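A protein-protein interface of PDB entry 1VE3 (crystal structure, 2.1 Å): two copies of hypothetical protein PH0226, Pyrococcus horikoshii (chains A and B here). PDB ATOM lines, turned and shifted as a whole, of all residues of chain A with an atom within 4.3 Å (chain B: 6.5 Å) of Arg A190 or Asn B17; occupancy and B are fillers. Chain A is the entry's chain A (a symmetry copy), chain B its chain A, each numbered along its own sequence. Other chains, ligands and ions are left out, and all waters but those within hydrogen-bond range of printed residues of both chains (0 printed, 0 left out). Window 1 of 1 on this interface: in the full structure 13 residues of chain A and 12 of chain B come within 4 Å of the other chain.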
ATOM      1  N   GLY A   2     -14.432   8.843  30.562  1.00  0.00           N
ATOM      2  CA  GLY A   2     -14.770   7.973  31.725  1.00  0.00           C
ATOM      3  C   GLY A   2     -16.124   8.346  32.291  1.00  0.00           C
ATOM      4  O   GLY A   2     -16.700   9.353  31.882  1.00  0.00           O
ATOM      5  N   GLU A 117     -12.635  16.427  24.686  1.00  0.00           N
ATOM      6  CA  GLU A 117     -12.502  16.327  23.241  1.00  0.00           C
ATOM      7  C   GLU A 117     -11.581  17.509  22.882  1.00  0.00           C
ATOM      8  O   GLU A 117     -11.314  18.368  23.728  1.00  0.00           O
ATOM      9  CB  GLU A 117     -13.866  16.438  22.554  1.00  0.00           C
ATOM     10  CG  GLU A 117     -14.545  17.786  22.639  1.00  0.00           C
ATOM     11  CD  GLU A 117     -15.876  17.803  21.899  1.00  0.00           C
ATOM     12  OE1 GLU A 117     -15.961  17.188  20.813  1.00  0.00           O
ATOM     13  OE2 GLU A 117     -16.829  18.435  22.388  1.00  0.00           O
ATOM     14  N   GLU A 173     -13.483  10.095  14.781  1.00  0.00           N
ATOM     15  CA  GLU A 173     -14.091  10.860  15.863  1.00  0.00           C
ATOM     16  C   GLU A 173     -13.097  11.031  17.013  1.00  0.00           C
ATOM     17  O   GLU A 173     -13.293  11.867  17.900  1.00  0.00           O
ATOM     18  CB  GLU A 173     -15.335  10.116  16.362  1.00  0.00           C
ATOM     19  CG  GLU A 173     -16.282  10.934  17.221  1.00  0.00           C
ATOM     20  CD  GLU A 173     -17.578  10.195  17.516  1.00  0.00           C
ATOM     21  OE1 GLU A 173     -17.554   9.216  18.296  1.00  0.00           O
ATOM     22  OE2 GLU A 173     -18.622  10.591  16.955  1.00  0.00           O
ATOM     23  N   THR A 175     -12.365   8.752  19.351  1.00  0.00           N
ATOM     24  CA  THR A 175     -12.938   8.201  20.576  1.00  0.00           C
ATOM     25  C   THR A 175     -12.909   6.686  20.505  1.00  0.00           C
ATOM     26  O   THR A 175     -12.651   6.111  19.449  1.00  0.00           O
ATOM     27  CB  THR A 175     -14.411   8.627  20.784  1.00  0.00           C
ATOM     28  OG1 THR A 175     -15.228   8.019  19.776  1.00  0.00           O
ATOM     29  CG2 THR A 175     -14.560  10.148  20.712  1.00  0.00           C
ATOM     30  N   VAL A 176     -13.185   6.040  21.630  1.00  0.00           N
ATOM     31  CA  VAL A 176     -13.186   4.586  21.672  1.00  0.00           C
ATOM     32  C   VAL A 176     -14.088   4.077  22.788  1.00  0.00           C
ATOM     33  O   VAL A 176     -14.176   4.680  23.862  1.00  0.00           O
ATOM     34  CB  VAL A 176     -11.757   4.028  21.894  1.00  0.00           C
ATOM     35  CG1 VAL A 176     -11.250   4.434  23.263  1.00  0.00           C
ATOM     36  CG2 VAL A 176     -11.760   2.517  21.760  1.00  0.00           C
ATOM     37  N   VAL A 177     -14.761   2.965  22.512  1.00  0.00           N
ATOM     38  CA  VAL A 177     -15.648   2.334  23.472  1.00  0.00           C
ATOM     39  C   VAL A 177     -14.979   1.067  23.976  1.00  0.00           C
ATOM     40  O   VAL A 177     -14.601   0.203  23.186  1.00  0.00           O
ATOM     41  CB  VAL A 177     -16.993   1.938  22.826  1.00  0.00           C
ATOM     42  CG1 VAL A 177     -17.891   1.285  23.861  1.00  0.00           C
ATOM     43  CG2 VAL A 177     -17.668   3.160  22.235  1.00  0.00           C
ATOM     44  N   VAL A 189     -17.757   2.200  28.360  1.00  0.00           N
ATOM     45  CA  VAL A 189     -17.275   3.553  28.590  1.00  0.00           C
ATOM     46  C   VAL A 189     -16.661   4.075  27.298  1.00  0.00           C
ATOM     47  O   VAL A 189     -15.968   3.338  26.599  1.00  0.00           O
ATOM     48  CB  VAL A 189     -16.183   3.596  29.687  1.00  0.00           C
ATOM     49  CG1 VAL A 189     -15.837   5.039  30.024  1.00  0.00           C
ATOM     50  CG2 VAL A 189     -16.655   2.855  30.928  1.00  0.00           C
ATOM     51  N   ARG A 190     -16.933   5.334  26.975  1.00  0.00           N
ATOM     52  CA  ARG A 190     -16.357   5.952  25.786  1.00  0.00           C
ATOM     53  C   ARG A 190     -15.299   6.954  26.249  1.00  0.00           C
ATOM     54  O   ARG A 190     -15.574   7.825  27.066  1.00  0.00           O
ATOM     55  CB  ARG A 190     -17.435   6.660  24.953  1.00  0.00           C
ATOM     56  CG  ARG A 190     -16.859   7.512  23.823  1.00  0.00           C
ATOM     57  CD  ARG A 190     -17.919   8.005  22.841  1.00  0.00           C
ATOM     58  NE  ARG A 190     -18.308   6.964  21.898  1.00  0.00           N
ATOM     59  CZ  ARG A 190     -19.409   6.229  21.993  1.00  0.00           C
ATOM     60  NH1 ARG A 190     -19.659   5.302  21.076  1.00  0.00           N
ATOM     61  NH2 ARG A 190     -20.268   6.431  22.990  1.00  0.00           N
ATOM     62  N   PHE A 191     -14.085   6.809  25.734  1.00  0.00           N
ATOM     63  CA  PHE A 191     -12.979   7.692  26.094  1.00  0.00           C
ATOM     64  C   PHE A 191     -12.560   8.531  24.899  1.00  0.00           C
ATOM     65  O   PHE A 191     -12.634   8.063  23.765  1.00  0.00           O
ATOM     66  CB  PHE A 191     -11.740   6.881  26.499  1.00  0.00           C
ATOM     67  CG  PHE A 191     -11.913   6.038  27.725  1.00  0.00           C
ATOM     68  CD1 PHE A 191     -11.906   6.613  28.989  1.00  0.00           C
ATOM     69  CD2 PHE A 191     -12.043   4.658  27.614  1.00  0.00           C
ATOM     70  CE1 PHE A 191     -12.024   5.819  30.132  1.00  0.00           C
ATOM     71  CE2 PHE A 191     -12.163   3.855  28.751  1.00  0.00           C
ATOM     72  CZ  PHE A 191     -12.153   4.437  30.012  1.00  0.00           C
ATOM     73  N   THR B  14     -26.015  19.343  20.386  1.00  0.00           N
ATOM     74  CA  THR B  14     -25.434  19.217  19.056  1.00  0.00           C
ATOM     75  C   THR B  14     -24.069  18.554  18.969  1.00  0.00           C
ATOM     76  O   THR B  14     -23.684  18.102  17.900  1.00  0.00           O
ATOM     77  CB  THR B  14     -25.359  20.591  18.365  1.00  0.00           C
ATOM     78  OG1 THR B  14     -24.655  21.514  19.208  1.00  0.00           O
ATOM     79  CG2 THR B  14     -26.761  21.121  18.107  1.00  0.00           C
ATOM     80  N   ASP B  15     -23.350  18.476  20.086  1.00  0.00           N
ATOM     81  CA  ASP B  15     -22.024  17.859  20.092  1.00  0.00           C
ATOM     82  C   ASP B  15     -22.011  16.591  20.937  1.00  0.00           C
ATOM     83  O   ASP B  15     -21.716  16.626  22.133  1.00  0.00           O
ATOM     84  CB  ASP B  15     -20.985  18.853  20.622  1.00  0.00           C
ATOM     85  CG  ASP B  15     -19.570  18.307  20.560  1.00  0.00           C
ATOM     86  OD1 ASP B  15     -19.390  17.121  20.214  1.00  0.00           O
ATOM     87  OD2 ASP B  15     -18.638  19.073  20.864  1.00  0.00           O
ATOM     88  N   ILE B  16     -22.318  15.469  20.291  1.00  0.00           N
ATOM     89  CA  ILE B  16     -22.390  14.165  20.945  1.00  0.00           C
ATOM     90  C   ILE B  16     -21.171  13.793  21.774  1.00  0.00           C
ATOM     91  O   ILE B  16     -21.280  12.985  22.691  1.00  0.00           O
ATOM     92  CB  ILE B  16     -22.655  13.035  19.908  1.00  0.00           C
ATOM     93  CG1 ILE B  16     -24.022  13.249  19.246  1.00  0.00           C
ATOM     94  CG2 ILE B  16     -22.641  11.674  20.591  1.00  0.00           C
ATOM     95  CD1 ILE B  16     -24.362  12.217  18.179  1.00  0.00           C
ATOM     96  N   ASN B  17     -20.014  14.371  21.473  1.00  0.00           N
ATOM     97  CA  ASN B  17     -18.814  14.050  22.249  1.00  0.00           C
ATOM     98  C   ASN B  17     -18.478  15.064  23.344  1.00  0.00           C
ATOM     99  O   ASN B  17     -17.497  14.895  24.070  1.00  0.00           O
ATOM    100  CB  ASN B  17     -17.612  13.869  21.323  1.00  0.00           C
ATOM    101  CG  ASN B  17     -17.715  12.611  20.485  1.00  0.00           C
ATOM    102  OD1 ASN B  17     -17.877  11.510  21.015  1.00  0.00           O
ATOM    103  ND2 ASN B  17     -17.620  12.766  19.168  1.00  0.00           N
ATOM    104  N   SER B  18     -19.291  16.111  23.475  1.00  0.00           N
ATOM    105  CA  SER B  18     -19.051  17.107  24.512  1.00  0.00           C
ATOM    106  C   SER B  18     -19.406  16.518  25.870  1.00  0.00           C
ATOM    107  O   SER B  18     -20.162  15.544  25.959  1.00  0.00           O
ATOM    108  CB  SER B  18     -19.904  18.353  24.279  1.00  0.00           C
ATOM    109  OG  SER B  18     -21.281  18.091  24.507  1.00  0.00           O
ATOM    110  N   GLN B  19     -18.854  17.110  26.928  1.00  0.00           N
ATOM    111  CA  GLN B  19     -19.139  16.647  28.278  1.00  0.00           C
ATOM    112  C   GLN B  19     -20.614  16.922  28.589  1.00  0.00           C
ATOM    113  O   GLN B  19     -21.260  16.146  29.291  1.00  0.00           O
ATOM    114  CB  GLN B  19     -18.240  17.363  29.299  1.00  0.00           C
ATOM    115  CG  GLN B  19     -16.739  17.110  29.120  1.00  0.00           C
ATOM    116  CD  GLN B  19     -15.881  17.757  30.209  1.00  0.00           C
ATOM    117  OE1 GLN B  19     -16.350  18.598  30.981  1.00  0.00           O
ATOM    118  NE2 GLN B  19     -14.613  17.373  30.261  1.00  0.00           N
ATOM    119  N   GLU B  20     -21.142  18.022  28.053  1.00  0.00           N
ATOM    120  CA  GLU B  20     -22.541  18.388  28.285  1.00  0.00           C
ATOM    121  C   GLU B  20     -23.493  17.302  27.786  1.00  0.00           C
ATOM    122  O   GLU B  20     -24.372  16.847  28.522  1.00  0.00           O
ATOM    123  CB  GLU B  20     -22.890  19.711  27.586  1.00  0.00           C
ATOM    124  CG  GLU B  20     -22.311  20.972  28.230  1.00  0.00           C
ATOM    125  CD  GLU B  20     -20.811  21.126  28.013  1.00  0.00           C
ATOM    126  OE1 GLU B  20     -20.253  20.400  27.162  1.00  0.00           O
ATOM    127  OE2 GLU B  20     -20.193  21.988  28.686  1.00  0.00           O
ATOM    128  N   TYR B  21     -23.302  16.889  26.535  1.00  0.00           N
ATOM    129  CA  TYR B  21     -24.131  15.868  25.904  1.00  0.00           C
ATOM    130  C   TYR B  21     -23.974  14.504  26.587  1.00  0.00           C
ATOM    131  O   TYR B  21     -24.963  13.804  26.832  1.00  0.00           O
ATOM    132  CB  TYR B  21     -23.755  15.768  24.422  1.00  0.00           C
ATOM    133  CG  TYR B  21     -24.856  15.306  23.483  1.00  0.00           C
ATOM    134  CD1 TYR B  21     -25.413  14.033  23.589  1.00  0.00           C
ATOM    135  CD2 TYR B  21     -25.298  16.132  22.450  1.00  0.00           C
ATOM    136  CE1 TYR B  21     -26.383  13.587  22.676  1.00  0.00           C
ATOM    137  CE2 TYR B  21     -26.264  15.703  21.537  1.00  0.00           C
ATOM    138  CZ  TYR B  21     -26.801  14.430  21.655  1.00  0.00           C
ATOM    139  OH  TYR B  21     -27.743  14.002  20.743  1.00  0.00           O
ATOM    140  N   ARG B  22     -22.734  14.125  26.892  1.00  0.00           N
ATOM    141  CA  ARG B  22     -22.469  12.842  27.537  1.00  0.00           C
ATOM    142  C   ARG B  22     -23.153  12.768  28.892  1.00  0.00           C
ATOM    143  O   ARG B  22     -23.672  11.723  29.278  1.00  0.00           O
ATOM    144  CB  ARG B  22     -20.964  12.620  27.703  1.00  0.00           C
ATOM    145  CG  ARG B  22     -20.232  12.392  26.390  1.00  0.00           C
ATOM    146  CD  ARG B  22     -18.752  12.093  26.619  1.00  0.00           C
ATOM    147  NE  ARG B  22     -18.109  11.637  25.388  1.00  0.00           N
ATOM    148  CZ  ARG B  22     -16.860  11.187  25.312  1.00  0.00           C
ATOM    149  NH1 ARG B  22     -16.103  11.129  26.401  1.00  0.00           N
ATOM    150  NH2 ARG B  22     -16.370  10.789  24.144  1.00  0.00           N
ATOM    151  N   ILE B  25     -26.709  11.799  28.411  1.00  0.00           N
ATOM    152  CA  ILE B  25     -26.819  10.390  28.064  1.00  0.00           C
ATOM    153  C   ILE B  25     -26.647   9.496  29.291  1.00  0.00           C
ATOM    154  O   ILE B  25     -27.509   8.674  29.602  1.00  0.00           O
ATOM    155  CB  ILE B  25     -25.767   9.996  26.994  1.00  0.00           C
ATOM    156  CG1 ILE B  25     -26.150  10.609  25.647  1.00  0.00           C
ATOM    157  CG2 ILE B  25     -25.657   8.484  26.886  1.00  0.00           C
ATOM    158  CD1 ILE B  25     -25.174  10.313  24.528  1.00  0.00           C
ATOM    159  N   GLU B  26     -25.543   9.673  30.004  1.00  0.00           N
ATOM    160  CA  GLU B  26     -25.266   8.845  31.168  1.00  0.00           C
ATOM    161  C   GLU B  26     -26.267   9.018  32.308  1.00  0.00           C
ATOM    162  O   GLU B  26     -26.395   8.149  33.172  1.00  0.00           O
ATOM    163  CB  GLU B  26     -23.835   9.103  31.647  1.00  0.00           C
ATOM    164  CG  GLU B  26     -22.811   8.941  30.526  1.00  0.00           C
ATOM    165  CD  GLU B  26     -21.373   9.048  30.995  1.00  0.00           C
ATOM    166  OE1 GLU B  26     -21.064   9.961  31.795  1.00  0.00           O
ATOM    167  OE2 GLU B  26     -20.546   8.224  30.549  1.00  0.00           O
ATOM    168  N   PHE B  54     -27.778   6.230  18.773  1.00  0.00           N
ATOM    169  CA  PHE B  54     -26.582   5.399  18.818  1.00  0.00           C
ATOM    170  C   PHE B  54     -26.535   4.620  20.127  1.00  0.00           C
ATOM    171  O   PHE B  54     -26.163   3.449  20.149  1.00  0.00           O
ATOM    172  CB  PHE B  54     -25.330   6.268  18.667  1.00  0.00           C
ATOM    173  CG  PHE B  54     -25.331   7.105  17.422  1.00  0.00           C
ATOM    174  CD1 PHE B  54     -25.621   6.529  16.187  1.00  0.00           C
ATOM    175  CD2 PHE B  54     -25.090   8.474  17.482  1.00  0.00           C
ATOM    176  CE1 PHE B  54     -25.678   7.299  15.036  1.00  0.00           C
ATOM    177  CE2 PHE B  54     -25.145   9.259  16.330  1.00  0.00           C
ATOM    178  CZ  PHE B  54     -25.442   8.667  15.102  1.00  0.00           C
ATOM    179  N   ASP B  58     -26.614   0.458  20.249  1.00  0.00           N
ATOM    180  CA  ASP B  58     -25.557  -0.361  20.839  1.00  0.00           C
ATOM    181  C   ASP B  58     -26.112  -1.341  21.863  1.00  0.00           C
ATOM    182  O   ASP B  58     -25.458  -2.323  22.216  1.00  0.00           O
ATOM    183  CB  ASP B  58     -24.494   0.519  21.503  1.00  0.00           C
ATOM    184  CG  ASP B  58     -23.889   1.524  20.547  1.00  0.00           C
ATOM    185  OD1 ASP B  58     -23.832   1.234  19.331  1.00  0.00           O
ATOM    186  OD2 ASP B  58     -23.459   2.601  21.014  1.00  0.00           O
ATOM    187  N   TYR B  79     -22.258  11.517  12.130  1.00  0.00           N
ATOM    188  CA  TYR B  79     -21.928  10.817  13.369  1.00  0.00           C
ATOM    189  C   TYR B  79     -22.129   9.325  13.171  1.00  0.00           C
ATOM    190  O   TYR B  79     -21.348   8.511  13.661  1.00  0.00           O
ATOM    191  CB  TYR B  79     -22.805  11.295  14.533  1.00  0.00           C
ATOM    192  CG  TYR B  79     -22.316  12.568  15.187  1.00  0.00           C
ATOM    193  CD1 TYR B  79     -21.025  12.651  15.714  1.00  0.00           C
ATOM    194  CD2 TYR B  79     -23.140  13.687  15.286  1.00  0.00           C
ATOM    195  CE1 TYR B  79     -20.567  13.818  16.327  1.00  0.00           C
ATOM    196  CE2 TYR B  79     -22.693  14.860  15.896  1.00  0.00           C
ATOM    197  CZ  TYR B  79     -21.405  14.918  16.415  1.00  0.00           C
ATOM    198  OH  TYR B  79     -20.960  16.070  17.031  1.00  0.00           O
ATOM    199  N   ARG B  83     -19.261   6.525  13.359  1.00  0.00           N
ATOM    200  CA  ARG B  83     -19.454   5.454  14.328  1.00  0.00           C
ATOM    201  C   ARG B  83     -19.886   4.164  13.648  1.00  0.00           C
ATOM    202  O   ARG B  83     -20.109   3.154  14.312  1.00  0.00           O
ATOM    203  CB  ARG B  83     -20.496   5.848  15.382  1.00  0.00           C
ATOM    204  CG  ARG B  83     -20.030   6.931  16.339  1.00  0.00           C
ATOM    205  CD  ARG B  83     -20.913   6.990  17.566  1.00  0.00           C
ATOM    206  NE  ARG B  83     -20.421   7.955  18.543  1.00  0.00           N
ATOM    207  CZ  ARG B  83     -20.971   8.150  19.737  1.00  0.00           C
ATOM    208  NH1 ARG B  83     -22.030   7.440  20.101  1.00  0.00           N
ATOM    209  NH2 ARG B  83     -20.469   9.061  20.561  1.00  0.00           N
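The side-chain amide nitrogen (ND2) of Asn B17 lies close to the side-chain carboxylate (OE2) of Glu A173, 3.3 Å away.
O of Arg A190 lies within hydrogen-bond range of NH1 of Arg B22 (3.4 Å).
OE1 of Glu A173 lies within salt-bridge range of NE of Arg B83.
The guanidinium group of Arg A190 lies close to the guanidinium group of Arg B83 (3.3 Å).
The side-chain carboxylate (OD2) of Asp B15 lies close to the side-chain carboxylate (OE2) of Glu A117.
OG of Ser B18 is in hydrogen-bond range of N of Tyr B21, 3.1 Å away.
OD1 of Asp B15 sits close to N of Asn B17 (3.1 Å).
The backbone carbonyl oxygen (O) of Asp B15 sits at hydrogen-bond distance from the side-chain hydroxyl (OG) of Ser B18, at 2.8 Å.
The side-chain carboxylate (OE1) of Glu A173 lies within hydrogen-bond range of the side-chain hydroxyl (OG1) of Thr A175, at 3.0 Å.
Glu A117 touches Asn B17.
Glu A117 touches Ser B18.
CD1 of Tyr B79 touches OE2 of Glu A173 (3.4 Å).
Asn B17 touches Thr A175.
Thr A175 touches Arg B22.
Arg A190 touches Asn B17 (CD to OD1, 3.95 Å).
Arg A190 touches just these residues of chain B: Asn B17, Arg B22 and Arg B83.
Of chain A, only Glu A117, Glu A173, Thr A175 and Arg A190 come within 4 Å of Asn B17.
Printed residues of chain B within 4 Å of Glu A117: Asp B15 (2.4 Å), Asn B17 (3.7 Å) and Ser B18 (3.3 Å).
Printed residues of chain B within 4 Å of Glu A173: Asn B17 (3.0 Å), Tyr B79 (3.4 Å) and Arg B83 (3.1 Å).
Printed residues of chain A within 4 Å of Arg B22: Thr A175 and Arg A190.
Of the printed residues of chain A, Ser B18 touches Glu A117 (3.3 Å).
Of the printed residues of chain A, Asp B15 touches Glu A117.
Phe A191 touches none of the printed residues of chain B.
No position is printed for both chains.
Of the 11 pairs that touch across the chains among the printed residues, none has its exchanged pair printed and touching as well.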
